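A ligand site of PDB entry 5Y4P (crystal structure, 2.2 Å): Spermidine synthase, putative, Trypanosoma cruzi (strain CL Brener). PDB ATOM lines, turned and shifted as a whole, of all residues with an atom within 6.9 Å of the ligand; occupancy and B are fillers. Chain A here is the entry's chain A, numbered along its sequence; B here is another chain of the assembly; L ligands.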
ATOM      1  N   GLU A  22      28.493  14.959  -1.219  1.00  0.00           N
ATOM      2  CA  GLU A  22      27.515  15.021  -2.313  1.00  0.00           C
ATOM      3  C   GLU A  22      26.771  16.351  -2.334  1.00  0.00           C
ATOM      4  O   GLU A  22      26.190  16.789  -1.326  1.00  0.00           O
ATOM      5  CB  GLU A  22      26.522  13.856  -2.253  1.00  0.00           C
ATOM      6  CG  GLU A  22      25.735  13.668  -3.536  1.00  0.00           C
ATOM      7  CD  GLU A  22      24.652  12.601  -3.468  1.00  0.00           C
ATOM      8  OE1 GLU A  22      24.382  12.060  -2.383  1.00  0.00           O
ATOM      9  OE2 GLU A  22      24.059  12.313  -4.542  1.00  0.00           O
ATOM     10  N   MET A  32      25.582  16.544   1.585  1.00  0.00           N
ATOM     11  CA  MET A  32      25.504  15.320   2.381  1.00  0.00           C
ATOM     12  C   MET A  32      26.873  14.624   2.382  1.00  0.00           C
ATOM     13  O   MET A  32      27.481  14.438   1.330  1.00  0.00           O
ATOM     14  CB  MET A  32      24.396  14.387   1.850  1.00  0.00           C
ATOM     15  CG  MET A  32      24.288  13.017   2.528  1.00  0.00           C
ATOM     16  SD  MET A  32      23.924  13.049   4.307  1.00  0.00           S
ATOM     17  CE  MET A  32      22.161  13.410   4.326  1.00  0.00           C
ATOM     18  N   SER A  33      27.337  14.223   3.562  1.00  0.00           N
ATOM     19  CA  SER A  33      28.664  13.663   3.680  1.00  0.00           C
ATOM     20  C   SER A  33      28.643  12.272   4.259  1.00  0.00           C
ATOM     21  O   SER A  33      27.943  12.008   5.221  1.00  0.00           O
ATOM     22  CB  SER A  33      29.565  14.576   4.509  1.00  0.00           C
ATOM     23  OG  SER A  33      29.788  15.756   3.790  1.00  0.00           O
ATOM     24  N   LEU A  34      29.399  11.376   3.625  1.00  0.00           N
ATOM     25  CA  LEU A  34      29.568  10.023   4.144  1.00  0.00           C
ATOM     26  C   LEU A  34      31.033   9.747   4.424  1.00  0.00           C
ATOM     27  O   LEU A  34      31.895  10.082   3.599  1.00  0.00           O
ATOM     28  CB  LEU A  34      29.005   8.993   3.159  1.00  0.00           C
ATOM     29  CG  LEU A  34      27.499   8.956   2.883  1.00  0.00           C
ATOM     30  CD1 LEU A  34      27.222   8.055   1.704  1.00  0.00           C
ATOM     31  CD2 LEU A  34      26.735   8.482   4.113  1.00  0.00           C
ATOM     32  N   TRP A  61      25.117   2.031   5.750  1.00  0.00           N
ATOM     33  CA  TRP A  61      25.167   2.204   4.301  1.00  0.00           C
ATOM     34  C   TRP A  61      25.836   1.092   3.466  1.00  0.00           C
ATOM     35  O   TRP A  61      25.451   0.877   2.293  1.00  0.00           O
ATOM     36  CB  TRP A  61      25.697   3.594   3.925  1.00  0.00           C
ATOM     37  CG  TRP A  61      24.830   4.615   4.552  1.00  0.00           C
ATOM     38  CD1 TRP A  61      25.115   5.378   5.643  1.00  0.00           C
ATOM     39  CD2 TRP A  61      23.491   4.939   4.163  1.00  0.00           C
ATOM     40  NE1 TRP A  61      24.033   6.174   5.942  1.00  0.00           N
ATOM     41  CE2 TRP A  61      23.019   5.916   5.051  1.00  0.00           C
ATOM     42  CE3 TRP A  61      22.641   4.496   3.131  1.00  0.00           C
ATOM     43  CZ2 TRP A  61      21.744   6.465   4.956  1.00  0.00           C
ATOM     44  CZ3 TRP A  61      21.361   5.045   3.024  1.00  0.00           C
ATOM     45  CH2 TRP A  61      20.930   6.021   3.932  1.00  0.00           C
ATOM     46  N   VAL A  64      29.036   1.865  -1.265  1.00  0.00           N
ATOM     47  CA  VAL A  64      28.373   2.987  -1.914  1.00  0.00           C
ATOM     48  C   VAL A  64      28.949   3.173  -3.315  1.00  0.00           C
ATOM     49  O   VAL A  64      30.163   3.203  -3.498  1.00  0.00           O
ATOM     50  CB  VAL A  64      28.573   4.291  -1.105  1.00  0.00           C
ATOM     51  CG1 VAL A  64      27.814   5.455  -1.744  1.00  0.00           C
ATOM     52  CG2 VAL A  64      28.179   4.093   0.356  1.00  0.00           C
ATOM     53  N   CYS A  70      27.352  11.801  -7.804  1.00  0.00           N
ATOM     54  CA  CYS A  70      25.986  11.567  -7.323  1.00  0.00           C
ATOM     55  C   CYS A  70      25.791  10.098  -6.984  1.00  0.00           C
ATOM     56  O   CYS A  70      25.810   9.248  -7.884  1.00  0.00           O
ATOM     57  CB  CYS A  70      24.955  11.993  -8.388  1.00  0.00           C
ATOM     58  SG  CYS A  70      24.975  13.764  -8.805  1.00  0.00           S
ATOM     59  N   ILE A  71      25.576   9.803  -5.694  1.00  0.00           N
ATOM     60  CA  ILE A  71      25.314   8.425  -5.234  1.00  0.00           C
ATOM     61  C   ILE A  71      24.154   7.842  -6.037  1.00  0.00           C
ATOM     62  O   ILE A  71      23.187   8.544  -6.320  1.00  0.00           O
ATOM     63  CB  ILE A  71      25.060   8.324  -3.703  1.00  0.00           C
ATOM     64  CG1 ILE A  71      26.367   8.555  -2.932  1.00  0.00           C
ATOM     65  CG2 ILE A  71      24.512   6.963  -3.312  1.00  0.00           C
ATOM     66  CD1 ILE A  71      26.198   9.233  -1.596  1.00  0.00           C
ATOM     67  N   GLN A  72      24.327   6.587  -6.469  1.00  0.00           N
ATOM     68  CA  GLN A  72      23.353   5.863  -7.291  1.00  0.00           C
ATOM     69  C   GLN A  72      22.952   4.583  -6.570  1.00  0.00           C
ATOM     70  O   GLN A  72      21.824   4.166  -6.716  1.00  0.00           O
ATOM     71  CB  GLN A  72      23.929   5.491  -8.674  1.00  0.00           C
ATOM     72  CG  GLN A  72      24.500   6.641  -9.484  1.00  0.00           C
ATOM     73  CD  GLN A  72      23.437   7.447 -10.220  1.00  0.00           C
ATOM     74  OE1 GLN A  72      22.519   6.882 -10.820  1.00  0.00           O
ATOM     75  NE2 GLN A  72      23.585   8.759 -10.190  1.00  0.00           N
ATOM     76  N   VAL A  73      23.886   3.965  -5.848  1.00  0.00           N
ATOM     77  CA  VAL A  73      23.650   2.668  -5.153  1.00  0.00           C
ATOM     78  C   VAL A  73      24.334   2.592  -3.784  1.00  0.00           C
ATOM     79  O   VAL A  73      25.533   2.883  -3.669  1.00  0.00           O
ATOM     80  CB  VAL A  73      24.145   1.440  -5.988  1.00  0.00           C
ATOM     81  CG1 VAL A  73      24.040   0.151  -5.180  1.00  0.00           C
ATOM     82  CG2 VAL A  73      23.347   1.285  -7.267  1.00  0.00           C
ATOM     83  N   THR A  74      23.559   2.205  -2.774  1.00  0.00           N
ATOM     84  CA  THR A  74      24.106   1.836  -1.453  1.00  0.00           C
ATOM     85  C   THR A  74      23.560   0.463  -1.154  1.00  0.00           C
ATOM     86  O   THR A  74      22.439   0.162  -1.605  1.00  0.00           O
ATOM     87  CB  THR A  74      23.699   2.798  -0.300  1.00  0.00           C
ATOM     88  OG1 THR A  74      22.383   2.493   0.191  1.00  0.00           O
ATOM     89  CG2 THR A  74      23.743   4.244  -0.735  1.00  0.00           C
ATOM     90  N   ASP A  77      19.858   0.867   0.983  1.00  0.00           N
ATOM     91  CA  ASP A  77      18.596   1.296   0.405  1.00  0.00           C
ATOM     92  C   ASP A  77      18.252   0.712  -0.978  1.00  0.00           C
ATOM     93  O   ASP A  77      17.156   0.967  -1.465  1.00  0.00           O
ATOM     94  CB  ASP A  77      18.476   2.845   0.404  1.00  0.00           C
ATOM     95  CG  ASP A  77      19.518   3.550  -0.486  1.00  0.00           C
ATOM     96  OD1 ASP A  77      20.319   2.884  -1.187  1.00  0.00           O
ATOM     97  OD2 ASP A  77      19.519   4.812  -0.469  1.00  0.00           O
ATOM     98  N   GLU A  78      19.153  -0.047  -1.614  1.00  0.00           N
ATOM     99  CA  GLU A  78      18.962  -0.409  -3.018  1.00  0.00           C
ATOM    100  C   GLU A  78      17.661  -1.163  -3.288  1.00  0.00           C
ATOM    101  O   GLU A  78      17.082  -1.027  -4.355  1.00  0.00           O
ATOM    102  CB  GLU A  78      20.186  -1.111  -3.633  1.00  0.00           C
ATOM    103  CG  GLU A  78      20.552  -2.445  -3.015  1.00  0.00           C
ATOM    104  CD  GLU A  78      19.785  -3.640  -3.563  1.00  0.00           C
ATOM    105  OE1 GLU A  78      19.982  -4.719  -2.972  1.00  0.00           O
ATOM    106  OE2 GLU A  78      19.008  -3.546  -4.558  1.00  0.00           O
ATOM    107  N   TYR A  81      14.360   1.478  -4.561  1.00  0.00           N
ATOM    108  CA  TYR A  81      14.263   1.856  -5.978  1.00  0.00           C
ATOM    109  C   TYR A  81      14.270   0.682  -6.956  1.00  0.00           C
ATOM    110  O   TYR A  81      13.621   0.761  -7.984  1.00  0.00           O
ATOM    111  CB  TYR A  81      15.275   2.954  -6.363  1.00  0.00           C
ATOM    112  CG  TYR A  81      16.630   2.850  -5.703  1.00  0.00           C
ATOM    113  CD1 TYR A  81      16.868   3.406  -4.413  1.00  0.00           C
ATOM    114  CD2 TYR A  81      17.684   2.216  -6.368  1.00  0.00           C
ATOM    115  CE1 TYR A  81      18.118   3.308  -3.816  1.00  0.00           C
ATOM    116  CE2 TYR A  81      18.942   2.122  -5.782  1.00  0.00           C
ATOM    117  CZ  TYR A  81      19.165   2.664  -4.517  1.00  0.00           C
ATOM    118  OH  TYR A  81      20.430   2.540  -3.972  1.00  0.00           O
ATOM    119  N   GLN A 209      12.915   6.487 -14.229  1.00  0.00           N
ATOM    120  CA  GLN A 209      13.302   7.206 -13.028  1.00  0.00           C
ATOM    121  C   GLN A 209      12.927   8.675 -13.164  1.00  0.00           C
ATOM    122  O   GLN A 209      13.414   9.367 -14.043  1.00  0.00           O
ATOM    123  CB  GLN A 209      14.783   7.001 -12.739  1.00  0.00           C
ATOM    124  CG  GLN A 209      15.017   5.669 -12.033  1.00  0.00           C
ATOM    125  CD  GLN A 209      14.944   5.791 -10.513  1.00  0.00           C
ATOM    126  OE1 GLN A 209      15.847   6.341  -9.883  1.00  0.00           O
ATOM    127  NE2 GLN A 209      13.884   5.253  -9.917  1.00  0.00           N
ATOM    128  N   VAL A 242      12.769   6.818   0.644  1.00  0.00           N
ATOM    129  CA  VAL A 242      14.202   6.514   0.738  1.00  0.00           C
ATOM    130  C   VAL A 242      14.683   6.981   2.131  1.00  0.00           C
ATOM    131  O   VAL A 242      14.139   7.957   2.672  1.00  0.00           O
ATOM    132  CB  VAL A 242      14.971   7.259  -0.364  1.00  0.00           C
ATOM    133  CG1 VAL A 242      16.422   6.803  -0.455  1.00  0.00           C
ATOM    134  CG2 VAL A 242      14.282   7.060  -1.698  1.00  0.00           C
ATOM    135  N   PRO A 243      15.659   6.266   2.758  1.00  0.00           N
ATOM    136  CA  PRO A 243      16.149   6.806   4.038  1.00  0.00           C
ATOM    137  C   PRO A 243      16.807   8.188   3.938  1.00  0.00           C
ATOM    138  O   PRO A 243      16.668   8.971   4.874  1.00  0.00           O
ATOM    139  CB  PRO A 243      17.126   5.733   4.566  1.00  0.00           C
ATOM    140  CG  PRO A 243      17.095   4.614   3.589  1.00  0.00           C
ATOM    141  CD  PRO A 243      16.056   4.866   2.529  1.00  0.00           C
ATOM    142  N   THR A 244      17.510   8.485   2.828  1.00  0.00           N
ATOM    143  CA  THR A 244      17.931   9.895   2.553  1.00  0.00           C
ATOM    144  C   THR A 244      17.926  10.366   1.072  1.00  0.00           C
ATOM    145  O   THR A 244      18.267   9.612   0.163  1.00  0.00           O
ATOM    146  CB  THR A 244      19.228  10.323   3.289  1.00  0.00           C
ATOM    147  OG1 THR A 244      19.408   9.566   4.494  1.00  0.00           O
ATOM    148  CG2 THR A 244      19.119  11.806   3.677  1.00  0.00           C
ATOM    149  N   TYR A 245      17.566  11.632   0.883  1.00  0.00           N
ATOM    150  CA  TYR A 245      17.265  12.257  -0.400  1.00  0.00           C
ATOM    151  C   TYR A 245      17.938  13.631  -0.537  1.00  0.00           C
ATOM    152  O   TYR A 245      18.415  14.016  -1.604  1.00  0.00           O
ATOM    153  CB  TYR A 245      15.724  12.417  -0.585  1.00  0.00           C
ATOM    154  CG  TYR A 245      14.841  12.144   0.642  1.00  0.00           C
ATOM    155  CD1 TYR A 245      15.197  12.604   1.935  1.00  0.00           C
ATOM    156  CD2 TYR A 245      13.622  11.452   0.513  1.00  0.00           C
ATOM    157  CE1 TYR A 245      14.379  12.343   3.041  1.00  0.00           C
ATOM    158  CE2 TYR A 245      12.793  11.208   1.609  1.00  0.00           C
ATOM    159  CZ  TYR A 245      13.174  11.649   2.868  1.00  0.00           C
ATOM    160  OH  TYR A 245      12.372  11.413   3.967  1.00  0.00           O
ATOM    161  N   ILE A 250      12.993  11.059  -4.803  1.00  0.00           N
ATOM    162  CA  ILE A 250      13.020  10.146  -5.953  1.00  0.00           C
ATOM    163  C   ILE A 250      11.692   9.372  -6.141  1.00  0.00           C
ATOM    164  O   ILE A 250      10.888   9.220  -5.212  1.00  0.00           O
ATOM    165  CB  ILE A 250      14.289   9.251  -5.931  1.00  0.00           C
ATOM    166  CG1 ILE A 250      14.981   9.233  -7.305  1.00  0.00           C
ATOM    167  CG2 ILE A 250      14.030   7.858  -5.349  1.00  0.00           C
ATOM    168  CD1 ILE A 250      16.277  10.030  -7.364  1.00  0.00           C
ATOM    169  N   TRP B  27      23.137   7.318  13.810  1.00  0.00           N
ATOM    170  CA  TRP B  27      23.624   7.112  12.441  1.00  0.00           C
ATOM    171  C   TRP B  27      25.031   7.694  12.195  1.00  0.00           C
ATOM    172  O   TRP B  27      25.173   8.780  11.619  1.00  0.00           O
ATOM    173  CB  TRP B  27      22.592   7.640  11.431  1.00  0.00           C
ATOM    174  CG  TRP B  27      21.664   6.590  10.876  1.00  0.00           C
ATOM    175  CD1 TRP B  27      21.504   5.301  11.322  1.00  0.00           C
ATOM    176  CD2 TRP B  27      20.731   6.744   9.793  1.00  0.00           C
ATOM    177  NE1 TRP B  27      20.555   4.654  10.581  1.00  0.00           N
ATOM    178  CE2 TRP B  27      20.065   5.510   9.634  1.00  0.00           C
ATOM    179  CE3 TRP B  27      20.405   7.804   8.943  1.00  0.00           C
ATOM    180  CZ2 TRP B  27      19.084   5.307   8.651  1.00  0.00           C
ATOM    181  CZ3 TRP B  27      19.429   7.607   7.966  1.00  0.00           C
ATOM    182  CH2 TRP B  27      18.777   6.364   7.823  1.00  0.00           C
ATOM    183  N   GLN B  30      27.754   9.891   8.877  1.00  0.00           N
ATOM    184  CA  GLN B  30      27.118  10.866   7.977  1.00  0.00           C
ATOM    185  C   GLN B  30      26.892  12.238   8.594  1.00  0.00           C
ATOM    186  O   GLN B  30      26.903  12.390   9.815  1.00  0.00           O
ATOM    187  CB  GLN B  30      25.821  10.322   7.326  1.00  0.00           C
ATOM    188  CG  GLN B  30      24.663  10.104   8.272  1.00  0.00           C
ATOM    189  CD  GLN B  30      23.548   9.349   7.620  1.00  0.00           C
ATOM    190  OE1 GLN B  30      22.810   9.887   6.782  1.00  0.00           O
ATOM    191  NE2 GLN B  30      23.394   8.096   8.001  1.00  0.00           N
ATOM    192  N   ALA B  31      26.707  13.229   7.729  1.00  0.00           N
ATOM    193  CA  ALA B  31      26.379  14.583   8.151  1.00  0.00           C
ATOM    194  C   ALA B  31      25.670  15.277   7.030  1.00  0.00           C
ATOM    195  O   ALA B  31      26.010  15.119   5.864  1.00  0.00           O
ATOM    196  CB  ALA B  31      27.628  15.369   8.513  1.00  0.00           C
ATOM    197  N   PRO B 246      18.097  13.584   7.601  1.00  0.00           N
ATOM    198  CA  PRO B 246      19.354  12.807   7.666  1.00  0.00           C
ATOM    199  C   PRO B 246      19.314  11.651   8.684  1.00  0.00           C
ATOM    200  O   PRO B 246      20.342  10.993   8.917  1.00  0.00           O
ATOM    201  CB  PRO B 246      20.389  13.869   8.066  1.00  0.00           C
ATOM    202  CG  PRO B 246      19.619  14.862   8.860  1.00  0.00           C
ATOM    203  CD  PRO B 246      18.238  14.901   8.266  1.00  0.00           C
HETATM  204  C1  LIG L   1      21.981   7.390   0.012  1.00  0.00           C
HETATM  205  C2  LIG L   1      22.655   7.832   1.135  1.00  0.00           C
HETATM  206  C3  LIG L   1      23.043   9.958   0.077  1.00  0.00           C
HETATM  207  C4  LIG L   1      21.833   8.217  -1.092  1.00  0.00           C
HETATM  208  C5  LIG L   1      23.181   9.124   1.162  1.00  0.00           C
HETATM  209  C6  LIG L   1      22.376   9.486  -1.034  1.00  0.00           C
HETATM  210  C7  LIG L   1      21.117   7.747  -2.290  1.00  0.00           C
HETATM  211  C8  LIG L   1      20.032   6.461  -3.739  1.00  0.00           C
HETATM  212  C9  LIG L   1      20.117   7.836  -4.369  1.00  0.00           C
HETATM  213  C10 LIG L   1      18.727   8.406  -4.483  1.00  0.00           C
HETATM  214  C11 LIG L   1      23.104   9.429   3.455  1.00  0.00           C
HETATM  215  N1  LIG L   1      20.710   6.517  -2.454  1.00  0.00           N
HETATM  216  N2  LIG L   1      20.803   8.581  -3.337  1.00  0.00           N
HETATM  217  O1  LIG L   1      22.253  10.317  -2.110  1.00  0.00           O
HETATM  218  O2  LIG L   1      23.887   9.622   2.264  1.00  0.00           O
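A nitrogen (N1) of the ligand sits close to the side-chain carboxylate of Asp 77, at 2.9 Å.
The side-chain carboxylate (OE1) of Glu 22 is in hydrogen-bond range of an oxygen (O1) of the ligand, at 2.8 Å.
The side-chain amide oxygen (OE1) of Gln 30 of chain B sits close to the backbone carbonyl oxygen (O) of Pro 246 of chain B (3.4 Å).
N of Ile 71 is in hydrogen-bond range of OE2 of Glu 22 (3.2 Å).
The side-chain hydroxyl (OH) of Tyr 81 lies within hydrogen-bond range of the side-chain carboxylate (OD1) of Asp 77, at 2.8 Å.
OH of Tyr 81 lies within hydrogen-bond range of N of Thr 74, 3.4 Å away.
The side-chain hydroxyl (OG1) of Thr 74 lies within hydrogen-bond range of the side-chain carboxylate (OD1) of Asp 77, 2.5 Å away.
O of Gln 72 is in hydrogen-bond range of OH of Tyr 81 (3.5 Å).
N of Glu 22 is in hydrogen-bond range of O of Met 32 (2.8 Å).
The side-chain amide nitrogen (NE2) of Gln 30 of chain B sits close to the indole nitrogen (NE1) of Trp 61, at 2.9 Å.
Met 32 touches the ligand.
CD2 of Leu 34 touches O2 of the ligand (3.6 Å).
CZ2 of Trp 61 touches C11 of the ligand, at 3.6 Å.
CG2 of Ile 71 touches C7 of the ligand, 3.6 Å away.
Thr 74 touches the ligand (CG2 to C1, 3.7 Å).
Tyr 81 touches the ligand (CE1 to C8, 3.7 Å).
Thr 244 touches the ligand (OG1 to C11, 3.8 Å).
Gln 30 of chain B touches the ligand.
The nearest printed residue that does not touch the ligand is Ile 250 (4.1 Å).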
